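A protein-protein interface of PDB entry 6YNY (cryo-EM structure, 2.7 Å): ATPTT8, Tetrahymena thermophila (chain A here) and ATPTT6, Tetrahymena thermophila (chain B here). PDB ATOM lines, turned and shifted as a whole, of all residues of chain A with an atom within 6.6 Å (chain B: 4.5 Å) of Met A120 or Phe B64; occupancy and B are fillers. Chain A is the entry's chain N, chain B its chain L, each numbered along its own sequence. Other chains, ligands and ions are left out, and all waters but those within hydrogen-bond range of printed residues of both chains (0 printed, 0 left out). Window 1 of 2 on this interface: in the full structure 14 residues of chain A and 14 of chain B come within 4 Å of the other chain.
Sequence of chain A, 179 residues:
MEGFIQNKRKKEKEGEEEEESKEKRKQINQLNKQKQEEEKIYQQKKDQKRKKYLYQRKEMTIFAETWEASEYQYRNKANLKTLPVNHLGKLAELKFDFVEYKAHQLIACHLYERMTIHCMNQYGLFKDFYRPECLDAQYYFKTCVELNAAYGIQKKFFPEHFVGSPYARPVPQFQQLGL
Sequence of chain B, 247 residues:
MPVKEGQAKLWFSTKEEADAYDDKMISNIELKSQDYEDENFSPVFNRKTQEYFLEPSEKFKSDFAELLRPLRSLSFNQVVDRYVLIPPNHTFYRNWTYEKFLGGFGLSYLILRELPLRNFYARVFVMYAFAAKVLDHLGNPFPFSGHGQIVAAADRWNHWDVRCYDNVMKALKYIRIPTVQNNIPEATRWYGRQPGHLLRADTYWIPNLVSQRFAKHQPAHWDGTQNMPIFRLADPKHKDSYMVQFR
Of the 16 printed residues of chain A, 5 touch a printed residue of chain B.
Hydrophobic or aromatic side chains of chain A within 4 Å of the printed part of chain B: Met A120, Leu A125 and Phe A126.
Of the 9 printed residues of chain B, 4 touch a printed residue of chain A.
Hydrophobic or aromatic side chains of chain B that line the printed part of chain A: Phe B60, Phe B64 and Leu B67.
Among the printed residues, no Asp or Glu carboxylate lies within 4 Å of a Lys or Arg side-chain nitrogen of the other chain.
Of chain B, only Phe B60 and Phe B64 come within 4 Å of Met A120.
Printed residues of chain B within 4 Å of Leu A125: Asp B63 (3.2 Å).
Of the printed residues of chain A, Asp B63 touches Gly A124 (3.1 Å), Leu A125 (3.2 Å) and Phe A126 (3.6 Å).
Of the printed residues of chain B, Gly A124 touches Asp B63 (3.1 Å).
Cys A134 touches none of the printed residues of chain B.
The nearest printed residue of chain B that does not touch Met A120 is Asp B63 (5.8 Å).
The nearest residue of chain A that does not touch Phe B64 is Leu A125 (4.3 Å).
Among the printed residues, pairs that only touch across the chains: Gly A124 with Asp B63 (3.1 Å), Asn A121 with Phe B60 (3.2 Å), Met A120 with Phe B60 (3.3 Å), Phe A126 with Asp B63 (3.6 Å), Phe A126 with Leu B67 (3.6 Å) and Met A120 with Phe B64 (3.7 Å).
OG of Ser B62 is in hydrogen-bond range of OD1 of Asp B63 (3.3 Å).
O of Ile A117 sits close to ND2 of Asn A121, 3.4 Å away.
The side-chain carboxylate (OD2) of Asp B63 is in hydrogen-bond range of the backbone NH (N) of Leu A125, 3.2 Å away.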
ATOM      1  N   PHE A  96       7.621  -4.299  38.701  1.00  0.00           N
ATOM      2  CA  PHE A  96       8.689  -5.184  39.129  1.00  0.00           C
ATOM      3  C   PHE A  96      10.047  -4.505  38.982  1.00  0.00           C
ATOM      4  O   PHE A  96      10.183  -3.434  38.388  1.00  0.00           O
ATOM      5  CB  PHE A  96       8.651  -6.485  38.332  1.00  0.00           C
ATOM      6  CG  PHE A  96       8.807  -6.296  36.855  1.00  0.00           C
ATOM      7  CD1 PHE A  96      10.051  -6.360  36.265  1.00  0.00           C
ATOM      8  CD2 PHE A  96       7.707  -6.055  36.056  1.00  0.00           C
ATOM      9  CE1 PHE A  96      10.194  -6.186  34.912  1.00  0.00           C
ATOM     10  CE2 PHE A  96       7.848  -5.878  34.704  1.00  0.00           C
ATOM     11  CZ  PHE A  96       9.091  -5.944  34.132  1.00  0.00           C
ATOM     12  N   MET A 115      11.552  -3.361  27.163  1.00  0.00           N
ATOM     13  CA  MET A 115      10.457  -3.421  28.121  1.00  0.00           C
ATOM     14  C   MET A 115       9.588  -4.645  27.877  1.00  0.00           C
ATOM     15  O   MET A 115       9.207  -5.345  28.822  1.00  0.00           O
ATOM     16  CB  MET A 115       9.624  -2.146  28.032  1.00  0.00           C
ATOM     17  CG  MET A 115      10.395  -0.884  28.354  1.00  0.00           C
ATOM     18  SD  MET A 115       9.610   0.605  27.720  1.00  0.00           S
ATOM     19  CE  MET A 115       8.027   0.499  28.528  1.00  0.00           C
ATOM     20  N   THR A 116       9.268  -4.922  26.615  1.00  0.00           N
ATOM     21  CA  THR A 116       8.483  -6.106  26.293  1.00  0.00           C
ATOM     22  C   THR A 116       9.178  -7.371  26.777  1.00  0.00           C
ATOM     23  O   THR A 116       8.525  -8.302  27.261  1.00  0.00           O
ATOM     24  CB  THR A 116       8.236  -6.170  24.787  1.00  0.00           C
ATOM     25  OG1 THR A 116       7.572  -4.977  24.356  1.00  0.00           O
ATOM     26  CG2 THR A 116       7.387  -7.358  24.434  1.00  0.00           C
ATOM     27  N   ILE A 117      10.503  -7.421  26.660  1.00  0.00           N
ATOM     28  CA  ILE A 117      11.254  -8.579  27.130  1.00  0.00           C
ATOM     29  C   ILE A 117      11.179  -8.682  28.646  1.00  0.00           C
ATOM     30  O   ILE A 117      10.896  -9.751  29.200  1.00  0.00           O
ATOM     31  CB  ILE A 117      12.709  -8.497  26.643  1.00  0.00           C
ATOM     32  CG1 ILE A 117      12.756  -8.465  25.119  1.00  0.00           C
ATOM     33  CG2 ILE A 117      13.507  -9.669  27.159  1.00  0.00           C
ATOM     34  CD1 ILE A 117      14.105  -8.128  24.562  1.00  0.00           C
ATOM     35  N   HIS A 118      11.442  -7.576  29.342  1.00  0.00           N
ATOM     36  CA  HIS A 118      11.344  -7.574  30.796  1.00  0.00           C
ATOM     37  C   HIS A 118       9.977  -8.056  31.259  1.00  0.00           C
ATOM     38  O   HIS A 118       9.871  -8.809  32.232  1.00  0.00           O
ATOM     39  CB  HIS A 118      11.619  -6.171  31.334  1.00  0.00           C
ATOM     40  CG  HIS A 118      13.057  -5.769  31.277  1.00  0.00           C
ATOM     41  ND1 HIS A 118      13.481  -4.619  30.648  1.00  0.00           N
ATOM     42  CD2 HIS A 118      14.168  -6.350  31.788  1.00  0.00           C
ATOM     43  CE1 HIS A 118      14.792  -4.516  30.762  1.00  0.00           C
ATOM     44  NE2 HIS A 118      15.234  -5.554  31.450  1.00  0.00           N
ATOM     45  N   CYS A 119       8.917  -7.627  30.574  1.00  0.00           N
ATOM     46  CA  CYS A 119       7.573  -8.035  30.961  1.00  0.00           C
ATOM     47  C   CYS A 119       7.293  -9.486  30.595  1.00  0.00           C
ATOM     48  O   CYS A 119       6.547 -10.167  31.305  1.00  0.00           O
ATOM     49  CB  CYS A 119       6.542  -7.113  30.314  1.00  0.00           C
ATOM     50  SG  CYS A 119       6.688  -5.385  30.793  1.00  0.00           S
ATOM     51  N   MET A 120       7.872  -9.974  29.500  1.00  0.00           N
ATOM     52  CA  MET A 120       7.700 -11.367  29.109  1.00  0.00           C
ATOM     53  C   MET A 120       8.569 -12.321  29.915  1.00  0.00           C
ATOM     54  O   MET A 120       8.356 -13.534  29.839  1.00  0.00           O
ATOM     55  CB  MET A 120       8.015 -11.540  27.624  1.00  0.00           C
ATOM     56  CG  MET A 120       6.974 -10.969  26.695  1.00  0.00           C
ATOM     57  SD  MET A 120       7.451 -11.090  24.968  1.00  0.00           S
ATOM     58  CE  MET A 120       5.995 -10.413  24.192  1.00  0.00           C
ATOM     59  N   ASN A 121       9.540 -11.811  30.668  1.00  0.00           N
ATOM     60  CA  ASN A 121      10.317 -12.634  31.583  1.00  0.00           C
ATOM     61  C   ASN A 121       9.665 -12.703  32.958  1.00  0.00           C
ATOM     62  O   ASN A 121       9.462 -13.792  33.500  1.00  0.00           O
ATOM     63  CB  ASN A 121      11.739 -12.091  31.706  1.00  0.00           C
ATOM     64  CG  ASN A 121      12.559 -12.324  30.464  1.00  0.00           C
ATOM     65  OD1 ASN A 121      12.263 -13.209  29.666  1.00  0.00           O
ATOM     66  ND2 ASN A 121      13.605 -11.536  30.298  1.00  0.00           N
ATOM     67  N   GLN A 122       9.337 -11.546  33.532  1.00  0.00           N
ATOM     68  CA  GLN A 122       8.634 -11.522  34.808  1.00  0.00           C
ATOM     69  C   GLN A 122       7.329 -12.294  34.704  1.00  0.00           C
ATOM     70  O   GLN A 122       7.088 -13.249  35.449  1.00  0.00           O
ATOM     71  CB  GLN A 122       8.376 -10.077  35.227  1.00  0.00           C
ATOM     72  CG  GLN A 122       7.709  -9.922  36.573  1.00  0.00           C
ATOM     73  CD  GLN A 122       8.610 -10.306  37.719  1.00  0.00           C
ATOM     74  OE1 GLN A 122       9.787 -10.603  37.528  1.00  0.00           O
ATOM     75  NE2 GLN A 122       8.059 -10.299  38.924  1.00  0.00           N
ATOM     76  N   TYR A 123       6.476 -11.885  33.779  1.00  0.00           N
ATOM     77  CA  TYR A 123       5.262 -12.604  33.455  1.00  0.00           C
ATOM     78  C   TYR A 123       5.520 -13.469  32.229  1.00  0.00           C
ATOM     79  O   TYR A 123       6.627 -13.516  31.691  1.00  0.00           O
ATOM     80  CB  TYR A 123       4.111 -11.629  33.217  1.00  0.00           C
ATOM     81  CG  TYR A 123       4.109 -10.456  34.165  1.00  0.00           C
ATOM     82  CD1 TYR A 123       4.535  -9.207  33.749  1.00  0.00           C
ATOM     83  CD2 TYR A 123       3.695 -10.600  35.477  1.00  0.00           C
ATOM     84  CE1 TYR A 123       4.539  -8.137  34.607  1.00  0.00           C
ATOM     85  CE2 TYR A 123       3.698  -9.532  36.342  1.00  0.00           C
ATOM     86  CZ  TYR A 123       4.122  -8.303  35.902  1.00  0.00           C
ATOM     87  OH  TYR A 123       4.128  -7.232  36.761  1.00  0.00           O
ATOM     88  N   GLY A 124       4.486 -14.166  31.786  1.00  0.00           N
ATOM     89  CA  GLY A 124       4.599 -14.987  30.600  1.00  0.00           C
ATOM     90  C   GLY A 124       3.882 -14.384  29.414  1.00  0.00           C
ATOM     91  O   GLY A 124       4.140 -13.240  29.032  1.00  0.00           O
ATOM     92  N   LEU A 125       2.986 -15.164  28.814  1.00  0.00           N
ATOM     93  CA  LEU A 125       2.151 -14.706  27.714  1.00  0.00           C
ATOM     94  C   LEU A 125       0.679 -15.023  27.946  1.00  0.00           C
ATOM     95  O   LEU A 125      -0.125 -14.875  27.020  1.00  0.00           O
ATOM     96  CB  LEU A 125       2.607 -15.338  26.393  1.00  0.00           C
ATOM     97  CG  LEU A 125       3.841 -14.786  25.677  1.00  0.00           C
ATOM     98  CD1 LEU A 125       3.636 -13.335  25.309  1.00  0.00           C
ATOM     99  CD2 LEU A 125       5.085 -14.947  26.513  1.00  0.00           C
ATOM    100  N   PHE A 126       0.302 -15.449  29.153  1.00  0.00           N
ATOM    101  CA  PHE A 126      -1.044 -15.951  29.412  1.00  0.00           C
ATOM    102  C   PHE A 126      -1.522 -15.465  30.774  1.00  0.00           C
ATOM    103  O   PHE A 126      -1.012 -15.908  31.808  1.00  0.00           O
ATOM    104  CB  PHE A 126      -1.078 -17.478  29.362  1.00  0.00           C
ATOM    105  CG  PHE A 126      -0.333 -18.069  28.207  1.00  0.00           C
ATOM    106  CD1 PHE A 126      -0.948 -18.251  26.984  1.00  0.00           C
ATOM    107  CD2 PHE A 126       0.983 -18.456  28.350  1.00  0.00           C
ATOM    108  CE1 PHE A 126      -0.258 -18.799  25.927  1.00  0.00           C
ATOM    109  CE2 PHE A 126       1.673 -19.006  27.299  1.00  0.00           C
ATOM    110  CZ  PHE A 126       1.051 -19.178  26.085  1.00  0.00           C
ATOM    111  N   PHE A 129       0.658 -11.488  31.558  1.00  0.00           N
ATOM    112  CA  PHE A 129       1.183 -10.441  30.698  1.00  0.00           C
ATOM    113  C   PHE A 129       0.101  -9.459  30.288  1.00  0.00           C
ATOM    114  O   PHE A 129       0.417  -8.351  29.845  1.00  0.00           O
ATOM    115  CB  PHE A 129       1.822 -11.074  29.464  1.00  0.00           C
ATOM    116  CG  PHE A 129       2.503 -10.099  28.566  1.00  0.00           C
ATOM    117  CD1 PHE A 129       3.766  -9.635  28.865  1.00  0.00           C
ATOM    118  CD2 PHE A 129       1.891  -9.658  27.415  1.00  0.00           C
ATOM    119  CE1 PHE A 129       4.396  -8.741  28.037  1.00  0.00           C
ATOM    120  CE2 PHE A 129       2.518  -8.765  26.588  1.00  0.00           C
ATOM    121  CZ  PHE A 129       3.772  -8.307  26.898  1.00  0.00           C
ATOM    122  N   CYS A 134       2.173  -3.701  30.311  1.00  0.00           N
ATOM    123  CA  CYS A 134       2.897  -4.608  29.432  1.00  0.00           C
ATOM    124  C   CYS A 134       2.342  -4.632  28.019  1.00  0.00           C
ATOM    125  O   CYS A 134       3.105  -4.823  27.066  1.00  0.00           O
ATOM    126  CB  CYS A 134       2.867  -6.026  30.001  1.00  0.00           C
ATOM    127  SG  CYS A 134       3.300  -6.149  31.741  1.00  0.00           S
ATOM    128  N   GLN A 138       4.247  -3.574  24.310  1.00  0.00           N
ATOM    129  CA  GLN A 138       4.242  -4.422  23.126  1.00  0.00           C
ATOM    130  C   GLN A 138       3.602  -3.712  21.942  1.00  0.00           C
ATOM    131  O   GLN A 138       4.077  -3.834  20.807  1.00  0.00           O
ATOM    132  CB  GLN A 138       3.515  -5.724  23.436  1.00  0.00           C
ATOM    133  CG  GLN A 138       3.568  -6.750  22.339  1.00  0.00           C
ATOM    134  CD  GLN A 138       2.713  -7.958  22.637  1.00  0.00           C
ATOM    135  OE1 GLN A 138       1.947  -7.969  23.596  1.00  0.00           O
ATOM    136  NE2 GLN A 138       2.841  -8.985  21.812  1.00  0.00           N
ATOM    137  N   PHE B  60      10.206 -17.264  29.198  1.00  0.00           N
ATOM    138  CA  PHE B  60      10.028 -16.556  27.938  1.00  0.00           C
ATOM    139  C   PHE B  60       9.965 -17.529  26.770  1.00  0.00           C
ATOM    140  O   PHE B  60       9.010 -17.519  25.988  1.00  0.00           O
ATOM    141  CB  PHE B  60      11.173 -15.564  27.762  1.00  0.00           C
ATOM    142  CG  PHE B  60      11.038 -14.666  26.573  1.00  0.00           C
ATOM    143  CD1 PHE B  60      11.393 -15.102  25.314  1.00  0.00           C
ATOM    144  CD2 PHE B  60      10.593 -13.370  26.722  1.00  0.00           C
ATOM    145  CE1 PHE B  60      11.281 -14.271  24.229  1.00  0.00           C
ATOM    146  CE2 PHE B  60      10.483 -12.538  25.639  1.00  0.00           C
ATOM    147  CZ  PHE B  60      10.829 -12.988  24.392  1.00  0.00           C
ATOM    148  N   LYS B  61      10.980 -18.384  26.640  1.00  0.00           N
ATOM    149  CA  LYS B  61      11.054 -19.303  25.515  1.00  0.00           C
ATOM    150  C   LYS B  61      10.087 -20.469  25.641  1.00  0.00           C
ATOM    151  O   LYS B  61       9.759 -21.093  24.627  1.00  0.00           O
ATOM    152  CB  LYS B  61      12.480 -19.835  25.370  1.00  0.00           C
ATOM    153  CG  LYS B  61      13.520 -18.747  25.172  1.00  0.00           C
ATOM    154  CD  LYS B  61      14.881 -19.320  24.820  1.00  0.00           C
ATOM    155  CE  LYS B  61      15.517 -20.042  25.988  1.00  0.00           C
ATOM    156  NZ  LYS B  61      15.844 -19.120  27.106  1.00  0.00           N
ATOM    157  N   SER B  62       9.627 -20.780  26.851  1.00  0.00           N
ATOM    158  CA  SER B  62       8.686 -21.877  27.021  1.00  0.00           C
ATOM    159  C   SER B  62       7.276 -21.476  26.618  1.00  0.00           C
ATOM    160  O   SER B  62       6.524 -22.307  26.098  1.00  0.00           O
ATOM    161  CB  SER B  62       8.698 -22.361  28.469  1.00  0.00           C
ATOM    162  OG  SER B  62       8.265 -21.343  29.349  1.00  0.00           O
ATOM    163  N   ASP B  63       6.901 -20.219  26.850  1.00  0.00           N
ATOM    164  CA  ASP B  63       5.564 -19.762  26.500  1.00  0.00           C
ATOM    165  C   ASP B  63       5.418 -19.510  25.005  1.00  0.00           C
ATOM    166  O   ASP B  63       4.335 -19.721  24.451  1.00  0.00           O
ATOM    167  CB  ASP B  63       5.221 -18.497  27.282  1.00  0.00           C
ATOM    168  CG  ASP B  63       5.010 -18.766  28.756  1.00  0.00           C
ATOM    169  OD1 ASP B  63       5.357 -19.874  29.214  1.00  0.00           O
ATOM    170  OD2 ASP B  63       4.484 -17.877  29.456  1.00  0.00           O
ATOM    171  N   PHE B  64       6.482 -19.061  24.339  1.00  0.00           N
ATOM    172  CA  PHE B  64       6.428 -18.933  22.889  1.00  0.00           C
ATOM    173  C   PHE B  64       6.328 -20.292  22.217  1.00  0.00           C
ATOM    174  O   PHE B  64       5.741 -20.405  21.135  1.00  0.00           O
ATOM    175  CB  PHE B  64       7.652 -18.182  22.372  1.00  0.00           C
ATOM    176  CG  PHE B  64       7.520 -16.696  22.441  1.00  0.00           C
ATOM    177  CD1 PHE B  64       6.744 -16.019  21.526  1.00  0.00           C
ATOM    178  CD2 PHE B  64       8.176 -15.975  23.413  1.00  0.00           C
ATOM    179  CE1 PHE B  64       6.620 -14.656  21.585  1.00  0.00           C
ATOM    180  CE2 PHE B  64       8.054 -14.611  23.474  1.00  0.00           C
ATOM    181  CZ  PHE B  64       7.276 -13.952  22.558  1.00  0.00           C
ATOM    182  N   ALA B  65       6.892 -21.328  22.833  1.00  0.00           N
ATOM    183  CA  ALA B  65       6.749 -22.679  22.316  1.00  0.00           C
ATOM    184  C   ALA B  65       5.397 -23.287  22.654  1.00  0.00           C
ATOM    185  O   ALA B  65       4.940 -24.187  21.943  1.00  0.00           O
ATOM    186  CB  ALA B  65       7.862 -23.566  22.866  1.00  0.00           C
ATOM    187  N   GLU B  66       4.753 -22.815  23.720  1.00  0.00           N
ATOM    188  CA  GLU B  66       3.426 -23.301  24.073  1.00  0.00           C
ATOM    189  C   GLU B  66       2.364 -22.787  23.114  1.00  0.00           C
ATOM    190  O   GLU B  66       1.297 -23.398  23.000  1.00  0.00           O
ATOM    191  CB  GLU B  66       3.087 -22.888  25.503  1.00  0.00           C
ATOM    192  CG  GLU B  66       1.818 -23.506  26.056  1.00  0.00           C
ATOM    193  CD  GLU B  66       1.926 -25.007  26.229  1.00  0.00           C
ATOM    194  OE1 GLU B  66       3.037 -25.550  26.057  1.00  0.00           O
ATOM    195  OE2 GLU B  66       0.899 -25.647  26.536  1.00  0.00           O
ATOM    196  N   LEU B  67       2.635 -21.676  22.428  1.00  0.00           N
ATOM    197  CA  LEU B  67       1.702 -21.164  21.434  1.00  0.00           C
ATOM    198  C   LEU B  67       1.664 -22.040  20.191  1.00  0.00           C
ATOM    199  O   LEU B  67       0.657 -22.051  19.475  1.00  0.00           O
ATOM    200  CB  LEU B  67       2.082 -19.737  21.050  1.00  0.00           C
ATOM    201  CG  LEU B  67       1.931 -18.656  22.114  1.00  0.00           C
ATOM    202  CD1 LEU B  67       2.605 -17.387  21.659  1.00  0.00           C
ATOM    203  CD2 LEU B  67       0.478 -18.391  22.401  1.00  0.00           C
ATOM    204  N   LEU B  68       2.740 -22.773  19.915  1.00  0.00           N
ATOM    205  CA  LEU B  68       2.849 -23.602  18.725  1.00  0.00           C
ATOM    206  C   LEU B  68       2.654 -25.081  19.016  1.00  0.00           C
ATOM    207  O   LEU B  68       2.987 -25.917  18.170  1.00  0.00           O
ATOM    208  CB  LEU B  68       4.206 -23.384  18.064  1.00  0.00           C
ATOM    209  CG  LEU B  68       4.567 -21.934  17.757  1.00  0.00           C
ATOM    210  CD1 LEU B  68       5.938 -21.870  17.139  1.00  0.00           C
ATOM    211  CD2 LEU B  68       3.547 -21.300  16.842  1.00  0.00           C
